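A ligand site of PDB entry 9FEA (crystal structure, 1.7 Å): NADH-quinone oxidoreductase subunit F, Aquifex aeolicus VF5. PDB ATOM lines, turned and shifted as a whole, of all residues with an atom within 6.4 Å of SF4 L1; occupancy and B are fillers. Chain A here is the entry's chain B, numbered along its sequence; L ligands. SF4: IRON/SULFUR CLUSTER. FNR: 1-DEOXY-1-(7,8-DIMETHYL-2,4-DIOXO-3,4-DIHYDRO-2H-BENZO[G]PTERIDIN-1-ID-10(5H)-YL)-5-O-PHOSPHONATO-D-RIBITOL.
An iron atom (FE4) of SF4 L1 is bound by the side-chain sulfur (SG) of Cys 353, at 2.3 Å.
The backbone NH of Gly 396 lies close to a sulfur (S3) of SF4 L1 (3.5 Å).
The backbone NH of Cys 347 lies close to a sulfur (S2) of SF4 L1 (3.6 Å).
A sulfur (S1) of SF4 L1 lies close to the backbone NH (N) of Cys 350, 3.2 Å away.
SG of Cys 393 is bound to FE1 of SF4 L1 (2.3 Å).
N of Cys 393 sits close to S3 of SF4 L1 (3.8 Å).
The side-chain hydroxyl (OG1) of Thr 346 sits close to a sulfur (S1) of SF4 L1 (3.6 Å).
The backbone NH (N) of Gly 348 lies close to a sulfur (S1) of SF4 L1 (3.5 Å).
An iron atom (FE3) of SF4 L1 is bound by the side-chain sulfur (SG) of Cys 347, at 2.3 Å.
FE2 of SF4 L1 is bound by SG of Cys 350.
The side-chain amide oxygen of Gln 349 lies close to a sulfur (S4) of SF4 L1 (3.5 Å).
A sulfur (S1) of SF4 L1 lies close to the backbone NH (N) of Gln 349 (3.3 Å).
The side-chain sulfur (SG) of Cys 350 lies close to the backbone NH (N) of Ile 392 (3.6 Å).
The backbone NH (N) of Gly 348 sits close to the side-chain hydroxyl (OG1) of Thr 346 (3.3 Å).
The side-chain amide oxygen (OE1) of Gln 349 sits close to the side-chain sulfur (SG) of Cys 347 (3.7 Å).
The backbone carbonyl oxygen (O) of Cys 353 lies close to the side-chain sulfur (SG) of Cys 357.
OG1 of Thr 346 sits close to SG of Cys 353, at 3.1 Å.
O of Pro 199 sits close to OE1 of Gln 349, at 2.9 Å.
The backbone NH (N) of Cys 353 lies within hydrogen-bond range of the backbone carbonyl oxygen (O) of Ile 387, at 3.4 Å.
The side-chain sulfur (SG) of Cys 393 sits close to the backbone NH (N) of Leu 395 (3.4 Å).
Ile 181 touches SF4 L1.
CG of Pro 199 touches S4 of SF4 L1, at 3.7 Å.
CB of Ser 391 touches S3 of SF4 L1, 3.6 Å away.
Ile 392 touches SF4 L1 (CG1 to S4, 3.4 Å).
Leu 395 touches SF4 L1.
Hydrophobic or aromatic side chains within 4 Å of SF4 L1: Ile 181, Pro 199, Ile 392 and Leu 395.
13 residues have an atom within 4 Å of SF4 L1: Ile 181, Pro 199, Thr 346, Cys 347, Gly 348, Gln 349, Cys 350, Cys 353, Ser 391, Ile 392, Cys 393, Leu 395 and Gly 396.
The nearest printed residue that does not touch SF4 L1 is Arg 354 (4.6 Å).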
ATOM      1  N   ILE A 181      14.994 -24.125  13.211  1.00  0.00           N
ATOM      2  CA  ILE A 181      14.638 -23.032  12.331  1.00  0.00           C
ATOM      3  C   ILE A 181      13.124 -22.898  12.284  1.00  0.00           C
ATOM      4  O   ILE A 181      12.638 -21.807  12.002  1.00  0.00           O
ATOM      5  CB  ILE A 181      15.271 -23.182  10.925  1.00  0.00           C
ATOM      6  CG1 ILE A 181      15.197 -21.914  10.101  1.00  0.00           C
ATOM      7  CG2 ILE A 181      14.664 -24.349  10.142  1.00  0.00           C
ATOM      8  CD1 ILE A 181      15.764 -20.691  10.797  1.00  0.00           C
ATOM      9  N   GLY A 197      10.864 -26.266   6.545  1.00  0.00           N
ATOM     10  CA  GLY A 197      10.949 -25.063   7.352  1.00  0.00           C
ATOM     11  C   GLY A 197      12.012 -24.108   6.791  1.00  0.00           C
ATOM     12  O   GLY A 197      13.120 -24.008   7.325  1.00  0.00           O
ATOM     13  N   HIS A 198      11.665 -23.441   5.698  1.00  0.00           N
ATOM     14  CA  HIS A 198      12.515 -22.463   5.043  1.00  0.00           C
ATOM     15  C   HIS A 198      11.956 -21.073   5.303  1.00  0.00           C
ATOM     16  O   HIS A 198      10.857 -20.764   4.836  1.00  0.00           O
ATOM     17  CB  HIS A 198      12.551 -22.726   3.541  1.00  0.00           C
ATOM     18  CG  HIS A 198      13.371 -23.889   3.168  1.00  0.00           C
ATOM     19  ND1 HIS A 198      13.335 -24.420   1.904  1.00  0.00           N
ATOM     20  CD2 HIS A 198      14.284 -24.585   3.820  1.00  0.00           C
ATOM     21  CE1 HIS A 198      14.195 -25.429   1.835  1.00  0.00           C
ATOM     22  NE2 HIS A 198      14.776 -25.547   2.978  1.00  0.00           N
ATOM     23  N   PRO A 199      12.658 -20.203   6.063  1.00  0.00           N
ATOM     24  CA  PRO A 199      12.200 -18.828   6.221  1.00  0.00           C
ATOM     25  C   PRO A 199      11.975 -18.123   4.885  1.00  0.00           C
ATOM     26  O   PRO A 199      12.638 -18.390   3.872  1.00  0.00           O
ATOM     27  CB  PRO A 199      13.337 -18.183   7.042  1.00  0.00           C
ATOM     28  CG  PRO A 199      13.905 -19.346   7.799  1.00  0.00           C
ATOM     29  CD  PRO A 199      13.919 -20.472   6.794  1.00  0.00           C
ATOM     30  N   ARG A 200      10.990 -17.216   4.943  1.00  0.00           N
ATOM     31  CA  ARG A 200      10.647 -16.363   3.817  1.00  0.00           C
ATOM     32  C   ARG A 200      11.301 -14.997   4.007  1.00  0.00           C
ATOM     33  O   ARG A 200      11.460 -14.531   5.136  1.00  0.00           O
ATOM     34  CB  ARG A 200       9.136 -16.109   3.785  1.00  0.00           C
ATOM     35  CG  ARG A 200       8.218 -17.324   3.804  1.00  0.00           C
ATOM     36  CD  ARG A 200       6.749 -16.897   3.897  1.00  0.00           C
ATOM     37  NE  ARG A 200       5.811 -18.030   3.844  1.00  0.00           N
ATOM     38  CZ  ARG A 200       4.482 -17.930   4.040  1.00  0.00           C
ATOM     39  NH1 ARG A 200       3.915 -16.781   4.377  1.00  0.00           N
ATOM     40  NH2 ARG A 200       3.725 -19.008   3.879  1.00  0.00           N
ATOM     41  N   GLU A 345      21.745 -26.479  12.482  1.00  0.00           N
ATOM     42  CA  GLU A 345      20.426 -25.848  12.363  1.00  0.00           C
ATOM     43  C   GLU A 345      20.283 -24.849  11.204  1.00  0.00           C
ATOM     44  O   GLU A 345      19.157 -24.509  10.863  1.00  0.00           O
ATOM     45  CB  GLU A 345      20.025 -25.164  13.673  1.00  0.00           C
ATOM     46  CG  GLU A 345      19.969 -26.134  14.845  1.00  0.00           C
ATOM     47  CD  GLU A 345      19.067 -27.344  14.695  1.00  0.00           C
ATOM     48  OE1 GLU A 345      18.140 -27.358  13.861  1.00  0.00           O
ATOM     49  OE2 GLU A 345      19.287 -28.322  15.450  1.00  0.00           O
ATOM     50  N   THR A 346      21.350 -24.469  10.498  1.00  0.00           N
ATOM     51  CA  THR A 346      21.141 -23.649   9.306  1.00  0.00           C
ATOM     52  C   THR A 346      20.273 -24.419   8.315  1.00  0.00           C
ATOM     53  O   THR A 346      20.489 -25.609   8.105  1.00  0.00           O
ATOM     54  CB  THR A 346      22.472 -23.233   8.656  1.00  0.00           C
ATOM     55  OG1 THR A 346      22.165 -22.576   7.410  1.00  0.00           O
ATOM     56  CG2 THR A 346      23.391 -24.412   8.386  1.00  0.00           C
ATOM     57  N   CYS A 347      19.293 -23.736   7.702  1.00  0.00           N
ATOM     58  CA  CYS A 347      18.393 -24.406   6.775  1.00  0.00           C
ATOM     59  C   CYS A 347      19.029 -24.497   5.384  1.00  0.00           C
ATOM     60  O   CYS A 347      18.571 -25.231   4.522  1.00  0.00           O
ATOM     61  CB  CYS A 347      17.033 -23.695   6.725  1.00  0.00           C
ATOM     62  SG  CYS A 347      16.988 -22.259   5.621  1.00  0.00           S
ATOM     63  N   GLY A 348      20.085 -23.695   5.130  1.00  0.00           N
ATOM     64  CA  GLY A 348      20.924 -23.811   3.958  1.00  0.00           C
ATOM     65  C   GLY A 348      20.479 -23.030   2.704  1.00  0.00           C
ATOM     66  O   GLY A 348      21.118 -23.141   1.687  1.00  0.00           O
ATOM     67  N   GLN A 349      19.423 -22.189   2.810  1.00  0.00           N
ATOM     68  CA  GLN A 349      18.932 -21.404   1.681  1.00  0.00           C
ATOM     69  C   GLN A 349      19.931 -20.321   1.258  1.00  0.00           C
ATOM     70  O   GLN A 349      20.005 -19.962   0.072  1.00  0.00           O
ATOM     71  CB  GLN A 349      17.688 -20.598   2.094  1.00  0.00           C
ATOM     72  CG  GLN A 349      16.396 -21.390   2.119  1.00  0.00           C
ATOM     73  CD  GLN A 349      15.227 -20.475   2.366  1.00  0.00           C
ATOM     74  OE1 GLN A 349      14.904 -20.079   3.498  1.00  0.00           O
ATOM     75  NE2 GLN A 349      14.608 -20.091   1.258  1.00  0.00           N
ATOM     76  N   CYS A 350      20.602 -19.725   2.249  1.00  0.00           N
ATOM     77  CA  CYS A 350      21.521 -18.639   2.002  1.00  0.00           C
ATOM     78  C   CYS A 350      22.947 -19.172   2.012  1.00  0.00           C
ATOM     79  O   CYS A 350      23.297 -19.987   2.865  1.00  0.00           O
ATOM     80  CB  CYS A 350      21.348 -17.546   3.069  1.00  0.00           C
ATOM     81  SG  CYS A 350      19.618 -17.209   3.432  1.00  0.00           S
ATOM     82  N   THR A 351      23.761 -18.706   1.054  1.00  0.00           N
ATOM     83  CA  THR A 351      25.060 -19.338   0.835  1.00  0.00           C
ATOM     84  C   THR A 351      26.016 -19.079   2.002  1.00  0.00           C
ATOM     85  O   THR A 351      26.568 -20.024   2.545  1.00  0.00           O
ATOM     86  CB  THR A 351      25.643 -18.965  -0.541  1.00  0.00           C
ATOM     87  OG1 THR A 351      24.896 -19.793  -1.439  1.00  0.00           O
ATOM     88  CG2 THR A 351      27.113 -19.310  -0.645  1.00  0.00           C
ATOM     89  N   CYS A 353      25.447 -18.326   5.111  1.00  0.00           N
ATOM     90  CA  CYS A 353      24.941 -19.053   6.272  1.00  0.00           C
ATOM     91  C   CYS A 353      25.214 -20.557   6.146  1.00  0.00           C
ATOM     92  O   CYS A 353      25.789 -21.167   7.043  1.00  0.00           O
ATOM     93  CB  CYS A 353      23.467 -18.740   6.481  1.00  0.00           C
ATOM     94  SG  CYS A 353      22.770 -19.590   7.923  1.00  0.00           S
ATOM     95  N   ARG A 354      24.823 -21.130   5.018  1.00  0.00           N
ATOM     96  CA  ARG A 354      25.015 -22.556   4.766  1.00  0.00           C
ATOM     97  C   ARG A 354      26.479 -22.939   4.934  1.00  0.00           C
ATOM     98  O   ARG A 354      26.788 -23.867   5.664  1.00  0.00           O
ATOM     99  CB  ARG A 354      24.557 -22.884   3.342  1.00  0.00           C
ATOM    100  CG  ARG A 354      24.675 -24.347   2.969  1.00  0.00           C
ATOM    101  CD  ARG A 354      24.177 -24.610   1.554  1.00  0.00           C
ATOM    102  NE  ARG A 354      24.983 -23.893   0.545  1.00  0.00           N
ATOM    103  CZ  ARG A 354      24.533 -22.908  -0.230  1.00  0.00           C
ATOM    104  NH1 ARG A 354      23.335 -22.371  -0.029  1.00  0.00           N
ATOM    105  NH2 ARG A 354      25.331 -22.460  -1.187  1.00  0.00           N
ATOM    106  N   CYS A 357      28.175 -21.509   8.667  1.00  0.00           N
ATOM    107  CA  CYS A 357      27.847 -22.279   9.875  1.00  0.00           C
ATOM    108  C   CYS A 357      28.606 -23.604   9.869  1.00  0.00           C
ATOM    109  O   CYS A 357      29.158 -24.041  10.895  1.00  0.00           O
ATOM    110  CB  CYS A 357      26.355 -22.562   9.985  1.00  0.00           C
ATOM    111  SG  CYS A 357      25.396 -21.087  10.398  1.00  0.00           S
ATOM    112  N   ILE A 387      29.193 -14.913   8.116  1.00  0.00           N
ATOM    113  CA  ILE A 387      28.038 -15.794   8.015  1.00  0.00           C
ATOM    114  C   ILE A 387      26.787 -14.993   7.630  1.00  0.00           C
ATOM    115  O   ILE A 387      25.921 -15.518   6.918  1.00  0.00           O
ATOM    116  CB  ILE A 387      27.822 -16.592   9.321  1.00  0.00           C
ATOM    117  CG1 ILE A 387      29.101 -17.322   9.761  1.00  0.00           C
ATOM    118  CG2 ILE A 387      26.615 -17.537   9.221  1.00  0.00           C
ATOM    119  CD1 ILE A 387      28.987 -18.114  11.063  1.00  0.00           C
ATOM    120  N   THR A 390      23.822 -11.573   3.040  1.00  0.00           N
ATOM    121  CA  THR A 390      22.707 -12.059   2.223  1.00  0.00           C
ATOM    122  C   THR A 390      21.707 -12.889   3.043  1.00  0.00           C
ATOM    123  O   THR A 390      20.690 -13.315   2.483  1.00  0.00           O
ATOM    124  CB  THR A 390      23.209 -12.818   0.992  1.00  0.00           C
ATOM    125  OG1 THR A 390      23.558 -14.151   1.362  1.00  0.00           O
ATOM    126  CG2 THR A 390      24.394 -12.144   0.318  1.00  0.00           C
ATOM    127  N   SER A 391      21.914 -13.080   4.357  1.00  0.00           N
ATOM    128  CA  SER A 391      21.024 -13.895   5.166  1.00  0.00           C
ATOM    129  C   SER A 391      19.622 -13.312   5.136  1.00  0.00           C
ATOM    130  O   SER A 391      19.429 -12.103   5.134  1.00  0.00           O
ATOM    131  CB  SER A 391      21.525 -14.021   6.593  1.00  0.00           C
ATOM    132  OG  SER A 391      21.684 -12.724   7.174  1.00  0.00           O
ATOM    133  N   ILE A 392      18.619 -14.193   5.101  1.00  0.00           N
ATOM    134  CA  ILE A 392      17.242 -13.728   5.087  1.00  0.00           C
ATOM    135  C   ILE A 392      16.574 -13.882   6.443  1.00  0.00           C
ATOM    136  O   ILE A 392      15.474 -13.356   6.602  1.00  0.00           O
ATOM    137  CB  ILE A 392      16.450 -14.370   3.931  1.00  0.00           C
ATOM    138  CG1 ILE A 392      16.392 -15.869   3.957  1.00  0.00           C
ATOM    139  CG2 ILE A 392      17.006 -13.885   2.598  1.00  0.00           C
ATOM    140  CD1 ILE A 392      15.636 -16.440   2.754  1.00  0.00           C
ATOM    141  N   CYS A 393      17.200 -14.566   7.386  1.00  0.00           N
ATOM    142  CA  CYS A 393      16.623 -14.672   8.731  1.00  0.00           C
ATOM    143  C   CYS A 393      17.669 -14.478   9.813  1.00  0.00           C
ATOM    144  O   CYS A 393      18.852 -14.338   9.569  1.00  0.00           O
ATOM    145  CB  CYS A 393      15.851 -15.970   8.943  1.00  0.00           C
ATOM    146  SG  CYS A 393      16.830 -17.339   9.601  1.00  0.00           S
ATOM    147  N   GLY A 394      17.197 -14.407  11.061  1.00  0.00           N
ATOM    148  CA  GLY A 394      18.060 -14.069  12.191  1.00  0.00           C
ATOM    149  C   GLY A 394      19.134 -15.110  12.504  1.00  0.00           C
ATOM    150  O   GLY A 394      20.098 -14.768  13.172  1.00  0.00           O
ATOM    151  N   LEU A 395      19.021 -16.351  12.002  1.00  0.00           N
ATOM    152  CA  LEU A 395      19.978 -17.366  12.335  1.00  0.00           C
ATOM    153  C   LEU A 395      21.326 -16.969  11.744  1.00  0.00           C
ATOM    154  O   LEU A 395      22.326 -16.962  12.447  1.00  0.00           O
ATOM    155  CB  LEU A 395      19.551 -18.770  11.899  1.00  0.00           C
ATOM    156  CG  LEU A 395      20.408 -19.923  12.428  1.00  0.00           C
ATOM    157  CD1 LEU A 395      19.601 -21.187  12.557  1.00  0.00           C
ATOM    158  CD2 LEU A 395      21.643 -20.200  11.544  1.00  0.00           C
ATOM    159  N   GLY A 396      21.335 -16.559  10.455  1.00  0.00           N
ATOM    160  CA  GLY A 396      22.588 -16.211   9.789  1.00  0.00           C
ATOM    161  C   GLY A 396      23.185 -14.953  10.397  1.00  0.00           C
ATOM    162  O   GLY A 396      24.395 -14.783  10.507  1.00  0.00           O
ATOM    163  N   ALA A 397      22.291 -14.084  10.875  1.00  0.00           N
ATOM    164  CA  ALA A 397      22.704 -12.817  11.469  1.00  0.00           C
ATOM    165  C   ALA A 397      23.421 -13.027  12.799  1.00  0.00           C
ATOM    166  O   ALA A 397      24.249 -12.192  13.138  1.00  0.00           O
ATOM    167  CB  ALA A 397      21.501 -11.909  11.634  1.00  0.00           C
HETATM  168 FE1  SF4 L   1      18.077 -18.233   7.904  1.00  0.00          FE
HETATM  169 FE2  SF4 L   1      19.202 -18.181   5.422  1.00  0.00          FE
HETATM  170 FE3  SF4 L   1      18.241 -20.550   6.404  1.00  0.00          FE
HETATM  171 FE4  SF4 L   1      20.531 -19.362   7.454  1.00  0.00          FE
HETATM  172  S1  SF4 L   1      20.273 -20.242   5.380  1.00  0.00           S
HETATM  173  S2  SF4 L   1      18.820 -20.334   8.617  1.00  0.00           S
HETATM  174  S3  SF4 L   1      19.952 -17.172   7.296  1.00  0.00           S
HETATM  175  S4  SF4 L   1      17.029 -18.594   5.907  1.00  0.00           S
HETATM  176  C9A FNR L   2      12.974 -17.490  16.452  1.00  0.00           C
HETATM  177  N10 FNR L   2      11.848 -17.075  17.218  1.00  0.00           N
HETATM  178  CAA FNR L   2      11.287 -17.977  18.090  1.00  0.00           C
HETATM  179  N1  FNR L   2      10.140 -17.586  18.733  1.00  0.00           N
HETATM  180  C2  FNR L   2       9.475 -18.419  19.584  1.00  0.00           C
HETATM  181  O2  FNR L   2       8.403 -18.077  20.097  1.00  0.00           O
HETATM  182  N3  FNR L   2      10.011 -19.651  19.779  1.00  0.00           N
HETATM  183  C4  FNR L   2      11.138 -20.173  19.157  1.00  0.00           C
HETATM  184  O4  FNR L   2      11.466 -21.325  19.381  1.00  0.00           O
HETATM  185  C4A FNR L   2      11.784 -19.232  18.282  1.00  0.00           C
HETATM  186  N5  FNR L   2      12.862 -19.664  17.544  1.00  0.00           N
HETATM  187  C5A FNR L   2      13.450 -18.801  16.619  1.00  0.00           C
HETATM  188  C6  FNR L   2      14.546 -19.244  15.869  1.00  0.00           C
HETATM  189  C7  FNR L   2      15.151 -18.384  14.954  1.00  0.00           C
HETATM  190  C7M FNR L   2      16.362 -18.863  14.184  1.00  0.00           C
HETATM  191  C8  FNR L   2      14.669 -17.074  14.795  1.00  0.00           C
HETATM  192  C8M FNR L   2      15.340 -16.092  13.877  1.00  0.00           C
HETATM  193  C9  FNR L   2      13.578 -16.630  15.537  1.00  0.00           C
HETATM  194  C1' FNR L   2      11.253 -15.754  17.032  1.00  0.00           C
HETATM  195  C2' FNR L   2      10.046 -15.796  16.096  1.00  0.00           C
HETATM  196  O2' FNR L   2      10.504 -15.692  14.744  1.00  0.00           O
HETATM  197  C3' FNR L   2       9.082 -14.657  16.421  1.00  0.00           C
HETATM  198  O3' FNR L   2       9.743 -13.415  16.615  1.00  0.00           O
HETATM  199  C4' FNR L   2       8.240 -14.865  17.673  1.00  0.00           C
HETATM  200  O4' FNR L   2       7.711 -16.174  17.735  1.00  0.00           O
HETATM  201  C5' FNR L   2       7.176 -13.795  17.739  1.00  0.00           C
HETATM  202  O5' FNR L   2       6.461 -13.921  18.992  1.00  0.00           O
HETATM  203  P   FNR L   2       6.636 -12.797  20.135  1.00  0.00           P
HETATM  204  O1P FNR L   2       6.424 -11.422  19.556  1.00  0.00           O
HETATM  205  O2P FNR L   2       5.582 -13.165  21.174  1.00  0.00           O
HETATM  206  O3P FNR L   2       8.043 -12.966  20.663  1.00  0.00           O
